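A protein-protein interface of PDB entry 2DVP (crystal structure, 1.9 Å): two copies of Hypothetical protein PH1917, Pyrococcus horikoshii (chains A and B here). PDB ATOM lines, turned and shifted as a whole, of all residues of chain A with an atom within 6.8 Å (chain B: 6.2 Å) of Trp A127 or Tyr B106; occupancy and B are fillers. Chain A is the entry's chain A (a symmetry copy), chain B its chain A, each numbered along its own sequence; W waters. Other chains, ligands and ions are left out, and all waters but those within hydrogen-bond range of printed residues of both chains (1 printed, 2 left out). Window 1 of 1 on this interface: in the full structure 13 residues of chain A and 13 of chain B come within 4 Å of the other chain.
Glu A71 touches Phe B69. CA of Gly B75 touches OE1 of Glu A71, at 3.5 Å. Arg A104 touches Phe B69 (NH2 to CE1, 3.8 Å). CZ3 of Trp B127 touches OH of Tyr A106 (3.2 Å). Tyr B106 touches Trp A127 (OH to CZ3, 3.2 Å). Trp A127 touches Lys B108. CH2 of Trp A127 touches CH2 of Trp B127, 3.9 Å away.
Of the printed residues of chain B, Glu A71 touches Phe B69 and Gly B75. Printed residues of chain B within 4 Å of Tyr A106: Trp B127 (3.2 Å). Of chain B, only Tyr B106 (3.2 Å), Lys B108 (3.2 Å) and Trp B127 (3.9 Å) come within 4 Å of Trp A127. Of the printed residues of chain A, Glu B43 touches Glu A149 (2.5 Å). Tyr B106 touches just one residue of chain A: Trp A127 (3.2 Å). Of the printed residues of chain A, Lys B108 touches Trp A127 (3.2 Å). Of the printed residues of chain A, Trp B127 touches Tyr A106 (3.2 Å) and Trp A127 (3.9 Å). The nearest printed residue of chain B that does not touch Arg A104 is Tyr B106 (4.1 Å).
Water W1 lies within hydrogen-bond range of the backbone carbonyl oxygen of Glu B71 and the backbone carbonyl oxygen of Glu A71.
Hydrophobic or aromatic side chains of chain B within 4 Å of the printed part of chain A: Phe B69, Tyr B106 and Trp B127. Among the printed residues, 8 pairs touch across the chains. Among the printed residues, no Asp or Glu carboxylate lies within 4 Å of a Lys or Arg side-chain nitrogen of the other chain.
OE2 of Glu B43 lies close to OE1 of Glu A149 (2.5 Å).
The backbone NH (N) of Glu A149 is in hydrogen-bond range of the backbone carbonyl oxygen (O) of Trp A127 (2.9 Å). The backbone NH (N) of Phe B69 is in hydrogen-bond range of the backbone carbonyl oxygen (O) of Tyr B106 (2.8 Å). N of Gly B67 is in hydrogen-bond range of O of Lys B108, 2.9 Å away. N of Gly B75 is in hydrogen-bond range of O of Ile B70 (3.0 Å). The side-chain carboxylate of Glu A71 is in salt-bridge range of the guanidinium group of Arg A104 (2.6 Å).
Tyr A106 touches Trp B127, and with the chains exchanged Trp A127 touches Tyr B106. Trp B127 touches its own counterpart, Trp A127.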
ATOM      1  N   GLU A  71     -21.946  17.510  -2.533  1.00  0.00           N
ATOM      2  CA  GLU A  71     -20.919  16.478  -2.313  1.00  0.00           C
ATOM      3  C   GLU A  71     -19.912  16.876  -1.259  1.00  0.00           C
ATOM      4  O   GLU A  71     -19.718  16.123  -0.340  1.00  0.00           O
ATOM      5  CB  GLU A  71     -20.194  16.118  -3.596  1.00  0.00           C
ATOM      6  CG  GLU A  71     -19.332  14.900  -3.440  1.00  0.00           C
ATOM      7  CD  GLU A  71     -18.754  14.353  -4.762  1.00  0.00           C
ATOM      8  OE1 GLU A  71     -18.982  13.157  -5.014  1.00  0.00           O
ATOM      9  OE2 GLU A  71     -18.093  15.105  -5.522  1.00  0.00           O
ATOM     10  N   ARG A 104     -19.664  19.850  -7.079  1.00  0.00           N
ATOM     11  CA  ARG A 104     -20.656  18.872  -7.497  1.00  0.00           C
ATOM     12  C   ARG A 104     -21.798  18.710  -6.506  1.00  0.00           C
ATOM     13  O   ARG A 104     -21.612  18.809  -5.295  1.00  0.00           O
ATOM     14  CB  ARG A 104     -20.022  17.495  -7.708  1.00  0.00           C
ATOM     15  CG  ARG A 104     -18.947  17.488  -8.749  1.00  0.00           C
ATOM     16  CD  ARG A 104     -18.895  16.234  -9.514  1.00  0.00           C
ATOM     17  NE  ARG A 104     -18.612  15.063  -8.693  1.00  0.00           N
ATOM     18  CZ  ARG A 104     -19.502  14.128  -8.333  1.00  0.00           C
ATOM     19  NH1 ARG A 104     -20.797  14.216  -8.644  1.00  0.00           N
ATOM     20  NH2 ARG A 104     -19.085  13.094  -7.629  1.00  0.00           N
ATOM     21  N   ALA A 105     -22.984  18.471  -7.049  1.00  0.00           N
ATOM     22  CA  ALA A 105     -24.168  18.294  -6.233  1.00  0.00           C
ATOM     23  C   ALA A 105     -25.183  17.564  -7.068  1.00  0.00           C
ATOM     24  O   ALA A 105     -25.027  17.466  -8.297  1.00  0.00           O
ATOM     25  CB  ALA A 105     -24.749  19.645  -5.776  1.00  0.00           C
ATOM     26  N   TYR A 106     -26.185  17.014  -6.399  1.00  0.00           N
ATOM     27  CA  TYR A 106     -27.375  16.504  -7.094  1.00  0.00           C
ATOM     28  C   TYR A 106     -28.672  16.958  -6.427  1.00  0.00           C
ATOM     29  O   TYR A 106     -28.723  17.192  -5.215  1.00  0.00           O
ATOM     30  CB  TYR A 106     -27.350  14.983  -7.223  1.00  0.00           C
ATOM     31  CG  TYR A 106     -27.459  14.204  -5.920  1.00  0.00           C
ATOM     32  CD1 TYR A 106     -28.689  13.809  -5.413  1.00  0.00           C
ATOM     33  CD2 TYR A 106     -26.324  13.843  -5.205  1.00  0.00           C
ATOM     34  CE1 TYR A 106     -28.775  13.110  -4.223  1.00  0.00           C
ATOM     35  CE2 TYR A 106     -26.413  13.135  -4.024  1.00  0.00           C
ATOM     36  CZ  TYR A 106     -27.605  12.776  -3.539  1.00  0.00           C
ATOM     37  OH  TYR A 106     -27.667  12.061  -2.383  1.00  0.00           O
ATOM     38  N   PHE A 107     -29.702  17.110  -7.259  1.00  0.00           N
ATOM     39  CA  PHE A 107     -31.087  17.223  -6.809  1.00  0.00           C
ATOM     40  C   PHE A 107     -31.749  15.847  -6.860  1.00  0.00           C
ATOM     41  O   PHE A 107     -31.539  15.022  -7.809  1.00  0.00           O
ATOM     42  CB  PHE A 107     -31.888  18.200  -7.673  1.00  0.00           C
ATOM     43  CG  PHE A 107     -31.952  19.609  -7.177  1.00  0.00           C
ATOM     44  CD1 PHE A 107     -32.662  19.929  -6.018  1.00  0.00           C
ATOM     45  CD2 PHE A 107     -31.405  20.632  -7.915  1.00  0.00           C
ATOM     46  CE1 PHE A 107     -32.783  21.224  -5.610  1.00  0.00           C
ATOM     47  CE2 PHE A 107     -31.517  21.942  -7.503  1.00  0.00           C
ATOM     48  CZ  PHE A 107     -32.196  22.240  -6.342  1.00  0.00           C
ATOM     49  N   VAL A 125     -33.393  11.945 -10.094  1.00  0.00           N
ATOM     50  CA  VAL A 125     -32.142  12.557  -9.657  1.00  0.00           C
ATOM     51  C   VAL A 125     -31.473  13.256 -10.812  1.00  0.00           C
ATOM     52  O   VAL A 125     -31.348  12.693 -11.914  1.00  0.00           O
ATOM     53  CB  VAL A 125     -31.181  11.502  -9.143  1.00  0.00           C
ATOM     54  CG1 VAL A 125     -29.795  12.113  -8.826  1.00  0.00           C
ATOM     55  CG2 VAL A 125     -31.753  10.744  -7.982  1.00  0.00           C
ATOM     56  N   THR A 126     -31.065  14.494 -10.597  1.00  0.00           N
ATOM     57  CA  THR A 126     -30.260  15.184 -11.598  1.00  0.00           C
ATOM     58  C   THR A 126     -28.971  15.673 -10.976  1.00  0.00           C
ATOM     59  O   THR A 126     -29.002  16.348  -9.933  1.00  0.00           O
ATOM     60  CB  THR A 126     -31.032  16.352 -12.186  1.00  0.00           C
ATOM     61  OG1 THR A 126     -32.159  15.831 -12.889  1.00  0.00           O
ATOM     62  CG2 THR A 126     -30.181  17.169 -13.138  1.00  0.00           C
ATOM     63  N   TRP A 127     -27.861  15.323 -11.624  1.00  0.00           N
ATOM     64  CA  TRP A 127     -26.523  15.665 -11.161  1.00  0.00           C
ATOM     65  C   TRP A 127     -26.151  16.980 -11.755  1.00  0.00           C
ATOM     66  O   TRP A 127     -26.649  17.356 -12.821  1.00  0.00           O
ATOM     67  CB  TRP A 127     -25.501  14.581 -11.575  1.00  0.00           C
ATOM     68  CG  TRP A 127     -25.949  13.221 -11.090  1.00  0.00           C
ATOM     69  CD1 TRP A 127     -26.858  12.384 -11.699  1.00  0.00           C
ATOM     70  CD2 TRP A 127     -25.598  12.596  -9.865  1.00  0.00           C
ATOM     71  NE1 TRP A 127     -27.059  11.262 -10.928  1.00  0.00           N
ATOM     72  CE2 TRP A 127     -26.295  11.367  -9.801  1.00  0.00           C
ATOM     73  CE3 TRP A 127     -24.744  12.948  -8.804  1.00  0.00           C
ATOM     74  CZ2 TRP A 127     -26.166  10.491  -8.730  1.00  0.00           C
ATOM     75  CZ3 TRP A 127     -24.624  12.080  -7.755  1.00  0.00           C
ATOM     76  CH2 TRP A 127     -25.339  10.884  -7.706  1.00  0.00           C
ATOM     77  N   GLY A 128     -25.248  17.679 -11.082  1.00  0.00           N
ATOM     78  CA  GLY A 128     -24.822  18.983 -11.521  1.00  0.00           C
ATOM     79  C   GLY A 128     -23.758  19.581 -10.635  1.00  0.00           C
ATOM     80  O   GLY A 128     -22.978  18.866  -9.992  1.00  0.00           O
ATOM     81  N   ARG A 129     -23.714  20.905 -10.652  1.00  0.00           N
ATOM     82  CA  ARG A 129     -22.777  21.695  -9.880  1.00  0.00           C
ATOM     83  C   ARG A 129     -23.400  23.001  -9.407  1.00  0.00           C
ATOM     84  O   ARG A 129     -24.338  23.529 -10.004  1.00  0.00           O
ATOM     85  CB  ARG A 129     -21.499  21.988 -10.671  1.00  0.00           C
ATOM     86  CG  ARG A 129     -21.655  22.886 -11.930  1.00  0.00           C
ATOM     87  CD  ARG A 129     -20.606  22.488 -13.014  1.00  0.00           C
ATOM     88  NE  ARG A 129     -20.998  22.765 -14.405  1.00  0.00           N
ATOM     89  CZ  ARG A 129     -22.074  22.238 -15.008  1.00  0.00           C
ATOM     90  NH1 ARG A 129     -22.936  21.435 -14.360  1.00  0.00           N
ATOM     91  NH2 ARG A 129     -22.317  22.526 -16.278  1.00  0.00           N
ATOM     92  N   PHE A 146     -27.987  26.170  -9.247  1.00  0.00           N
ATOM     93  CA  PHE A 146     -27.758  24.806  -9.736  1.00  0.00           C
ATOM     94  C   PHE A 146     -27.741  24.724 -11.267  1.00  0.00           C
ATOM     95  O   PHE A 146     -28.745  25.053 -11.930  1.00  0.00           O
ATOM     96  CB  PHE A 146     -28.825  23.852  -9.224  1.00  0.00           C
ATOM     97  CG  PHE A 146     -28.564  22.419  -9.552  1.00  0.00           C
ATOM     98  CD1 PHE A 146     -27.666  21.653  -8.780  1.00  0.00           C
ATOM     99  CD2 PHE A 146     -29.234  21.801 -10.611  1.00  0.00           C
ATOM    100  CE1 PHE A 146     -27.423  20.338  -9.081  1.00  0.00           C
ATOM    101  CE2 PHE A 146     -29.020  20.465 -10.896  1.00  0.00           C
ATOM    102  CZ  PHE A 146     -28.118  19.725 -10.139  1.00  0.00           C
ATOM    103  N   ILE A 147     -26.633  24.216 -11.793  1.00  0.00           N
ATOM    104  CA  ILE A 147     -26.517  23.918 -13.222  1.00  0.00           C
ATOM    105  C   ILE A 147     -26.428  22.423 -13.445  1.00  0.00           C
ATOM    106  O   ILE A 147     -25.444  21.799 -13.051  1.00  0.00           O
ATOM    107  CB  ILE A 147     -25.255  24.534 -13.827  1.00  0.00           C
ATOM    108  CG1 ILE A 147     -25.138  26.020 -13.473  1.00  0.00           C
ATOM    109  CG2 ILE A 147     -25.261  24.295 -15.354  1.00  0.00           C
ATOM    110  CD1 ILE A 147     -23.671  26.522 -13.504  1.00  0.00           C
ATOM    111  N   PRO A 148     -27.438  21.839 -14.106  1.00  0.00           N
ATOM    112  CA  PRO A 148     -27.407  20.412 -14.293  1.00  0.00           C
ATOM    113  C   PRO A 148     -26.339  20.020 -15.314  1.00  0.00           C
ATOM    114  O   PRO A 148     -25.898  20.847 -16.121  1.00  0.00           O
ATOM    115  CB  PRO A 148     -28.827  20.091 -14.782  1.00  0.00           C
ATOM    116  CG  PRO A 148     -29.269  21.300 -15.477  1.00  0.00           C
ATOM    117  CD  PRO A 148     -28.624  22.449 -14.747  1.00  0.00           C
ATOM    118  N   GLU A 149     -25.900  18.776 -15.217  1.00  0.00           N
ATOM    119  CA  GLU A 149     -24.843  18.239 -16.060  1.00  0.00           C
ATOM    120  C   GLU A 149     -25.316  18.342 -17.507  1.00  0.00           C
ATOM    121  O   GLU A 149     -26.469  18.012 -17.814  1.00  0.00           O
ATOM    122  CB  GLU A 149     -24.568  16.779 -15.680  1.00  0.00           C
ATOM    123  CG  GLU A 149     -23.105  16.443 -15.421  1.00  0.00           C
ATOM    124  CD  GLU A 149     -22.904  15.428 -14.267  1.00  0.00           C
ATOM    125  OE1 GLU A 149     -23.390  14.277 -14.382  1.00  0.00           O
ATOM    126  OE2 GLU A 149     -22.237  15.790 -13.257  1.00  0.00           O
ATOM    127  N   GLY A 150     -24.437  18.820 -18.375  1.00  0.00           N
ATOM    128  CA  GLY A 150     -24.743  18.909 -19.813  1.00  0.00           C
ATOM    129  C   GLY A 150     -25.288  20.250 -20.256  1.00  0.00           C
ATOM    130  O   GLY A 150     -25.408  20.517 -21.463  1.00  0.00           O
ATOM    131  N   LEU A 166     -35.276  18.285 -17.770  1.00  0.00           N
ATOM    132  CA  LEU A 166     -33.940  18.048 -17.204  1.00  0.00           C
ATOM    133  C   LEU A 166     -33.922  17.741 -15.689  1.00  0.00           C
ATOM    134  O   LEU A 166     -32.982  17.087 -15.198  1.00  0.00           O
ATOM    135  CB  LEU A 166     -33.057  19.265 -17.464  1.00  0.00           C
ATOM    136  CG  LEU A 166     -32.632  19.507 -18.911  1.00  0.00           C
ATOM    137  CD1 LEU A 166     -31.868  20.814 -19.035  1.00  0.00           C
ATOM    138  CD2 LEU A 166     -31.788  18.342 -19.435  1.00  0.00           C
ATOM    139  N   LYS A 171     -38.099  13.809 -13.632  1.00  0.00           N
ATOM    140  CA  LYS A 171     -37.763  12.398 -13.784  1.00  0.00           C
ATOM    141  C   LYS A 171     -38.620  11.528 -12.890  1.00  0.00           C
ATOM    142  O   LYS A 171     -38.941  10.409 -13.239  1.00  0.00           O
ATOM    143  CB  LYS A 171     -36.254  12.107 -13.555  1.00  0.00           C
ATOM    144  CG  LYS A 171     -35.293  12.766 -14.540  1.00  0.00           C
ATOM    145  CD  LYS A 171     -33.814  12.712 -14.101  1.00  0.00           C
ATOM    146  CE  LYS A 171     -32.884  13.304 -15.136  1.00  0.00           C
ATOM    147  NZ  LYS A 171     -31.404  13.366 -14.788  1.00  0.00           N
ATOM    148  N   GLU B  43     -18.192   9.919 -16.018  1.00  0.00           N
ATOM    149  CA  GLU B  43     -18.407  10.151 -17.452  1.00  0.00           C
ATOM    150  C   GLU B  43     -17.233  10.835 -18.156  1.00  0.00           C
ATOM    151  O   GLU B  43     -16.956  10.541 -19.314  1.00  0.00           O
ATOM    152  CB  GLU B  43     -19.708  10.904 -17.734  1.00  0.00           C
ATOM    153  CG  GLU B  43     -19.853  12.259 -17.072  1.00  0.00           C
ATOM    154  CD  GLU B  43     -21.300  12.661 -16.956  1.00  0.00           C
ATOM    155  OE1 GLU B  43     -22.106  12.248 -17.828  1.00  0.00           O
ATOM    156  OE2 GLU B  43     -21.638  13.387 -16.000  1.00  0.00           O
ATOM    157  N   GLY B  67     -17.878   3.353  -9.585  1.00  0.00           N
ATOM    158  CA  GLY B  67     -17.301   3.722  -8.285  1.00  0.00           C
ATOM    159  C   GLY B  67     -18.323   3.741  -7.190  1.00  0.00           C
ATOM    160  O   GLY B  67     -19.532   3.846  -7.453  1.00  0.00           O
ATOM    161  N   LEU B  68     -17.819   3.611  -5.972  1.00  0.00           N
ATOM    162  CA  LEU B  68     -18.583   3.718  -4.756  1.00  0.00           C
ATOM    163  C   LEU B  68     -18.292   5.113  -4.179  1.00  0.00           C
ATOM    164  O   LEU B  68     -17.115   5.488  -4.056  1.00  0.00           O
ATOM    165  CB  LEU B  68     -18.171   2.626  -3.767  1.00  0.00           C
ATOM    166  CG  LEU B  68     -18.735   2.700  -2.339  1.00  0.00           C
ATOM    167  CD1 LEU B  68     -20.234   2.450  -2.352  1.00  0.00           C
ATOM    168  CD2 LEU B  68     -18.012   1.726  -1.358  1.00  0.00           C
ATOM    169  N   PHE B  69     -19.361   5.868  -3.890  1.00  0.00           N
ATOM    170  CA  PHE B  69     -19.276   7.268  -3.446  1.00  0.00           C
ATOM    171  C   PHE B  69     -19.901   7.330  -2.071  1.00  0.00           C
ATOM    172  O   PHE B  69     -21.101   7.078  -1.919  1.00  0.00           O
ATOM    173  CB  PHE B  69     -20.008   8.199  -4.415  1.00  0.00           C
ATOM    174  CG  PHE B  69     -19.409   8.238  -5.803  1.00  0.00           C
ATOM    175  CD1 PHE B  69     -18.722   9.369  -6.241  1.00  0.00           C
ATOM    176  CD2 PHE B  69     -19.523   7.155  -6.679  1.00  0.00           C
ATOM    177  CE1 PHE B  69     -18.193   9.431  -7.486  1.00  0.00           C
ATOM    178  CE2 PHE B  69     -18.991   7.219  -7.924  1.00  0.00           C
ATOM    179  CZ  PHE B  69     -18.316   8.347  -8.343  1.00  0.00           C
ATOM    180  N   ILE B  70     -19.092   7.633  -1.056  1.00  0.00           N
ATOM    181  CA  ILE B  70     -19.550   7.519   0.326  1.00  0.00           C
ATOM    182  C   ILE B  70     -19.849   8.950   0.857  1.00  0.00           C
ATOM    183  O   ILE B  70     -18.993   9.840   0.855  1.00  0.00           O
ATOM    184  CB  ILE B  70     -18.565   6.781   1.254  1.00  0.00           C
ATOM    185  CG1 ILE B  70     -18.365   5.326   0.770  1.00  0.00           C
ATOM    186  CG2 ILE B  70     -19.094   6.787   2.728  1.00  0.00           C
ATOM    187  CD1 ILE B  70     -17.212   4.610   1.399  1.00  0.00           C
ATOM    188  N   GLU B  71     -21.103   9.141   1.224  1.00  0.00           N
ATOM    189  CA  GLU B  71     -21.641  10.470   1.557  1.00  0.00           C
ATOM    190  C   GLU B  71     -20.804  11.194   2.587  1.00  0.00           C
ATOM    191  O   GLU B  71     -20.413  12.303   2.329  1.00  0.00           O
ATOM    192  CB  GLU B  71     -23.079  10.397   2.034  1.00  0.00           C
ATOM    193  CG  GLU B  71     -23.716  11.752   2.132  1.00  0.00           C
ATOM    194  CD  GLU B  71     -25.238  11.725   2.387  1.00  0.00           C
ATOM    195  OE1 GLU B  71     -25.946  12.351   1.580  1.00  0.00           O
ATOM    196  OE2 GLU B  71     -25.702  11.091   3.369  1.00  0.00           O
ATOM    197  N   GLY B  75     -17.734  11.787  -1.090  1.00  0.00           N
ATOM    198  CA  GLY B  75     -17.721  11.122  -2.399  1.00  0.00           C
ATOM    199  C   GLY B  75     -16.635  10.122  -2.591  1.00  0.00           C
ATOM    200  O   GLY B  75     -16.626   9.406  -3.594  1.00  0.00           O
ATOM    201  N   ARG B 104     -24.468   6.142   4.546  1.00  0.00           N
ATOM    202  CA  ARG B 104     -25.032   6.174   3.204  1.00  0.00           C
ATOM    203  C   ARG B 104     -23.980   6.281   2.112  1.00  0.00           C
ATOM    204  O   ARG B 104     -22.946   6.923   2.279  1.00  0.00           O
ATOM    205  CB  ARG B 104     -25.999   7.348   3.039  1.00  0.00           C
ATOM    206  CG  ARG B 104     -27.155   7.306   3.990  1.00  0.00           C
ATOM    207  CD  ARG B 104     -28.397   7.837   3.409  1.00  0.00           C
ATOM    208  NE  ARG B 104     -28.303   9.237   3.014  1.00  0.00           N
ATOM    209  CZ  ARG B 104     -28.207   9.688   1.756  1.00  0.00           C
ATOM    210  NH1 ARG B 104     -28.115   8.869   0.707  1.00  0.00           N
ATOM    211  NH2 ARG B 104     -28.183  10.991   1.551  1.00  0.00           N
ATOM    212  N   ALA B 105     -24.264   5.626   0.993  1.00  0.00           N
ATOM    213  CA  ALA B 105     -23.358   5.634  -0.138  1.00  0.00           C
ATOM    214  C   ALA B 105     -24.159   5.260  -1.354  1.00  0.00           C
ATOM    215  O   ALA B 105     -25.291   4.764  -1.230  1.00  0.00           O
ATOM    216  CB  ALA B 105     -22.206   4.630   0.052  1.00  0.00           C
ATOM    217  N   TYR B 106     -23.594   5.543  -2.519  1.00  0.00           N
ATOM    218  CA  TYR B 106     -24.132   5.003  -3.776  1.00  0.00           C
ATOM    219  C   TYR B 106     -23.036   4.427  -4.671  1.00  0.00           C
ATOM    220  O   TYR B 106     -21.882   4.864  -4.635  1.00  0.00           O
ATOM    221  CB  TYR B 106     -24.946   6.044  -4.539  1.00  0.00           C
ATOM    222  CG  TYR B 106     -24.165   7.232  -5.082  1.00  0.00           C
ATOM    223  CD1 TYR B 106     -23.613   7.214  -6.356  1.00  0.00           C
ATOM    224  CD2 TYR B 106     -23.998   8.384  -4.326  1.00  0.00           C
ATOM    225  CE1 TYR B 106     -22.897   8.297  -6.834  1.00  0.00           C
ATOM    226  CE2 TYR B 106     -23.293   9.467  -4.810  1.00  0.00           C
ATOM    227  CZ  TYR B 106     -22.752   9.430  -6.032  1.00  0.00           C
ATOM    228  OH  TYR B 106     -22.078  10.517  -6.496  1.00  0.00           O
ATOM    229  N   PHE B 107     -23.425   3.412  -5.442  1.00  0.00           N
ATOM    230  CA  PHE B 107     -22.650   2.928  -6.582  1.00  0.00           C
ATOM    231  C   PHE B 107     -23.164   3.588  -7.860  1.00  0.00           C
ATOM    232  O   PHE B 107     -24.404   3.787  -8.076  1.00  0.00           O
ATOM    233  CB  PHE B 107     -22.743   1.407  -6.729  1.00  0.00           C
ATOM    234  CG  PHE B 107     -21.657   0.620  -6.068  1.00  0.00           C
ATOM    235  CD1 PHE B 107     -20.346   0.665  -6.549  1.00  0.00           C
ATOM    236  CD2 PHE B 107     -21.950  -0.249  -5.045  1.00  0.00           C
ATOM    237  CE1 PHE B 107     -19.373  -0.112  -5.994  1.00  0.00           C
ATOM    238  CE2 PHE B 107     -20.970  -1.031  -4.474  1.00  0.00           C
ATOM    239  CZ  PHE B 107     -19.675  -0.955  -4.940  1.00  0.00           C
ATOM    240  N   LYS B 108     -22.223   3.972  -8.710  1.00  0.00           N
ATOM    241  CA  LYS B 108     -22.549   4.509 -10.045  1.00  0.00           C
ATOM    242  C   LYS B 108     -21.719   3.790 -11.092  1.00  0.00           C
ATOM    243  O   LYS B 108     -20.492   3.559 -10.895  1.00  0.00           O
ATOM    244  CB  LYS B 108     -22.282   6.001 -10.166  1.00  0.00           C
ATOM    245  CG  LYS B 108     -22.732   6.625 -11.466  1.00  0.00           C
ATOM    246  CD  LYS B 108     -22.536   8.154 -11.510  1.00  0.00           C
ATOM    247  CE  LYS B 108     -23.666   8.925 -10.877  1.00  0.00           C
ATOM    248  NZ  LYS B 108     -23.499  10.417 -11.030  1.00  0.00           N
ATOM    249  N   VAL B 125     -27.315   3.966 -11.177  1.00  0.00           N
ATOM    250  CA  VAL B 125     -26.967   4.327  -9.807  1.00  0.00           C
ATOM    251  C   VAL B 125     -27.796   3.530  -8.832  1.00  0.00           C
ATOM    252  O   VAL B 125     -29.026   3.422  -8.980  1.00  0.00           O
ATOM    253  CB  VAL B 125     -27.248   5.796  -9.552  1.00  0.00           C
ATOM    254  CG1 VAL B 125     -27.036   6.156  -8.063  1.00  0.00           C
ATOM    255  CG2 VAL B 125     -26.465   6.682 -10.475  1.00  0.00           C
ATOM    256  N   THR B 126     -27.144   2.937  -7.849  1.00  0.00           N
ATOM    257  CA  THR B 126     -27.878   2.290  -6.768  1.00  0.00           C
ATOM    258  C   THR B 126     -27.438   2.853  -5.435  1.00  0.00           C
ATOM    259  O   THR B 126     -26.229   2.894  -5.147  1.00  0.00           O
ATOM    260  CB  THR B 126     -27.655   0.789  -6.801  1.00  0.00           C
ATOM    261  OG1 THR B 126     -28.219   0.281  -8.009  1.00  0.00           O
ATOM    262  CG2 THR B 126     -28.301   0.097  -5.617  1.00  0.00           C
ATOM    263  N   TRP B 127     -28.424   3.278  -4.646  1.00  0.00           N
ATOM    264  CA  TRP B 127     -28.198   3.887  -3.343  1.00  0.00           C
ATOM    265  C   TRP B 127     -28.192   2.802  -2.322  1.00  0.00           C
ATOM    266  O   TRP B 127     -28.808   1.749  -2.514  1.00  0.00           O
ATOM    267  CB  TRP B 127     -29.300   4.923  -3.019  1.00  0.00           C
ATOM    268  CG  TRP B 127     -29.401   5.949  -4.124  1.00  0.00           C
ATOM    269  CD1 TRP B 127     -30.083   5.819  -5.314  1.00  0.00           C
ATOM    270  CD2 TRP B 127     -28.727   7.197  -4.191  1.00  0.00           C
ATOM    271  NE1 TRP B 127     -29.890   6.935  -6.095  1.00  0.00           N
ATOM    272  CE2 TRP B 127     -29.067   7.795  -5.427  1.00  0.00           C
ATOM    273  CE3 TRP B 127     -27.869   7.886  -3.316  1.00  0.00           C
ATOM    274  CZ2 TRP B 127     -28.587   9.042  -5.809  1.00  0.00           C
ATOM    275  CZ3 TRP B 127     -27.401   9.111  -3.701  1.00  0.00           C
ATOM    276  CH2 TRP B 127     -27.734   9.671  -4.935  1.00  0.00           C
ATOM    277  N   GLY B 128     -27.518   3.062  -1.211  1.00  0.00           N
ATOM    278  CA  GLY B 128     -27.398   2.090  -0.155  1.00  0.00           C
ATOM    279  C   GLY B 128     -26.626   2.609   1.033  1.00  0.00           C
ATOM    280  O   GLY B 128     -26.597   3.817   1.306  1.00  0.00           O
ATOM    281  N   PHE B 146     -21.380  -3.361   0.796  1.00  0.00           N
ATOM    282  CA  PHE B 146     -22.480  -2.528   0.300  1.00  0.00           C
ATOM    283  C   PHE B 146     -23.829  -3.255   0.325  1.00  0.00           C
ATOM    284  O   PHE B 146     -23.998  -4.298  -0.338  1.00  0.00           O
ATOM    285  CB  PHE B 146     -22.220  -2.064  -1.124  1.00  0.00           C
ATOM    286  CG  PHE B 146     -23.222  -1.081  -1.634  1.00  0.00           C
ATOM    287  CD1 PHE B 146     -23.135   0.284  -1.292  1.00  0.00           C
ATOM    288  CD2 PHE B 146     -24.247  -1.494  -2.490  1.00  0.00           C
ATOM    289  CE1 PHE B 146     -24.056   1.186  -1.757  1.00  0.00           C
ATOM    290  CE2 PHE B 146     -25.156  -0.582  -2.991  1.00  0.00           C
ATOM    291  CZ  PHE B 146     -25.071   0.760  -2.632  1.00  0.00           C
HETATM  292  O   HOH W   1     -21.034  13.623  -0.100  1.00  0.00           O
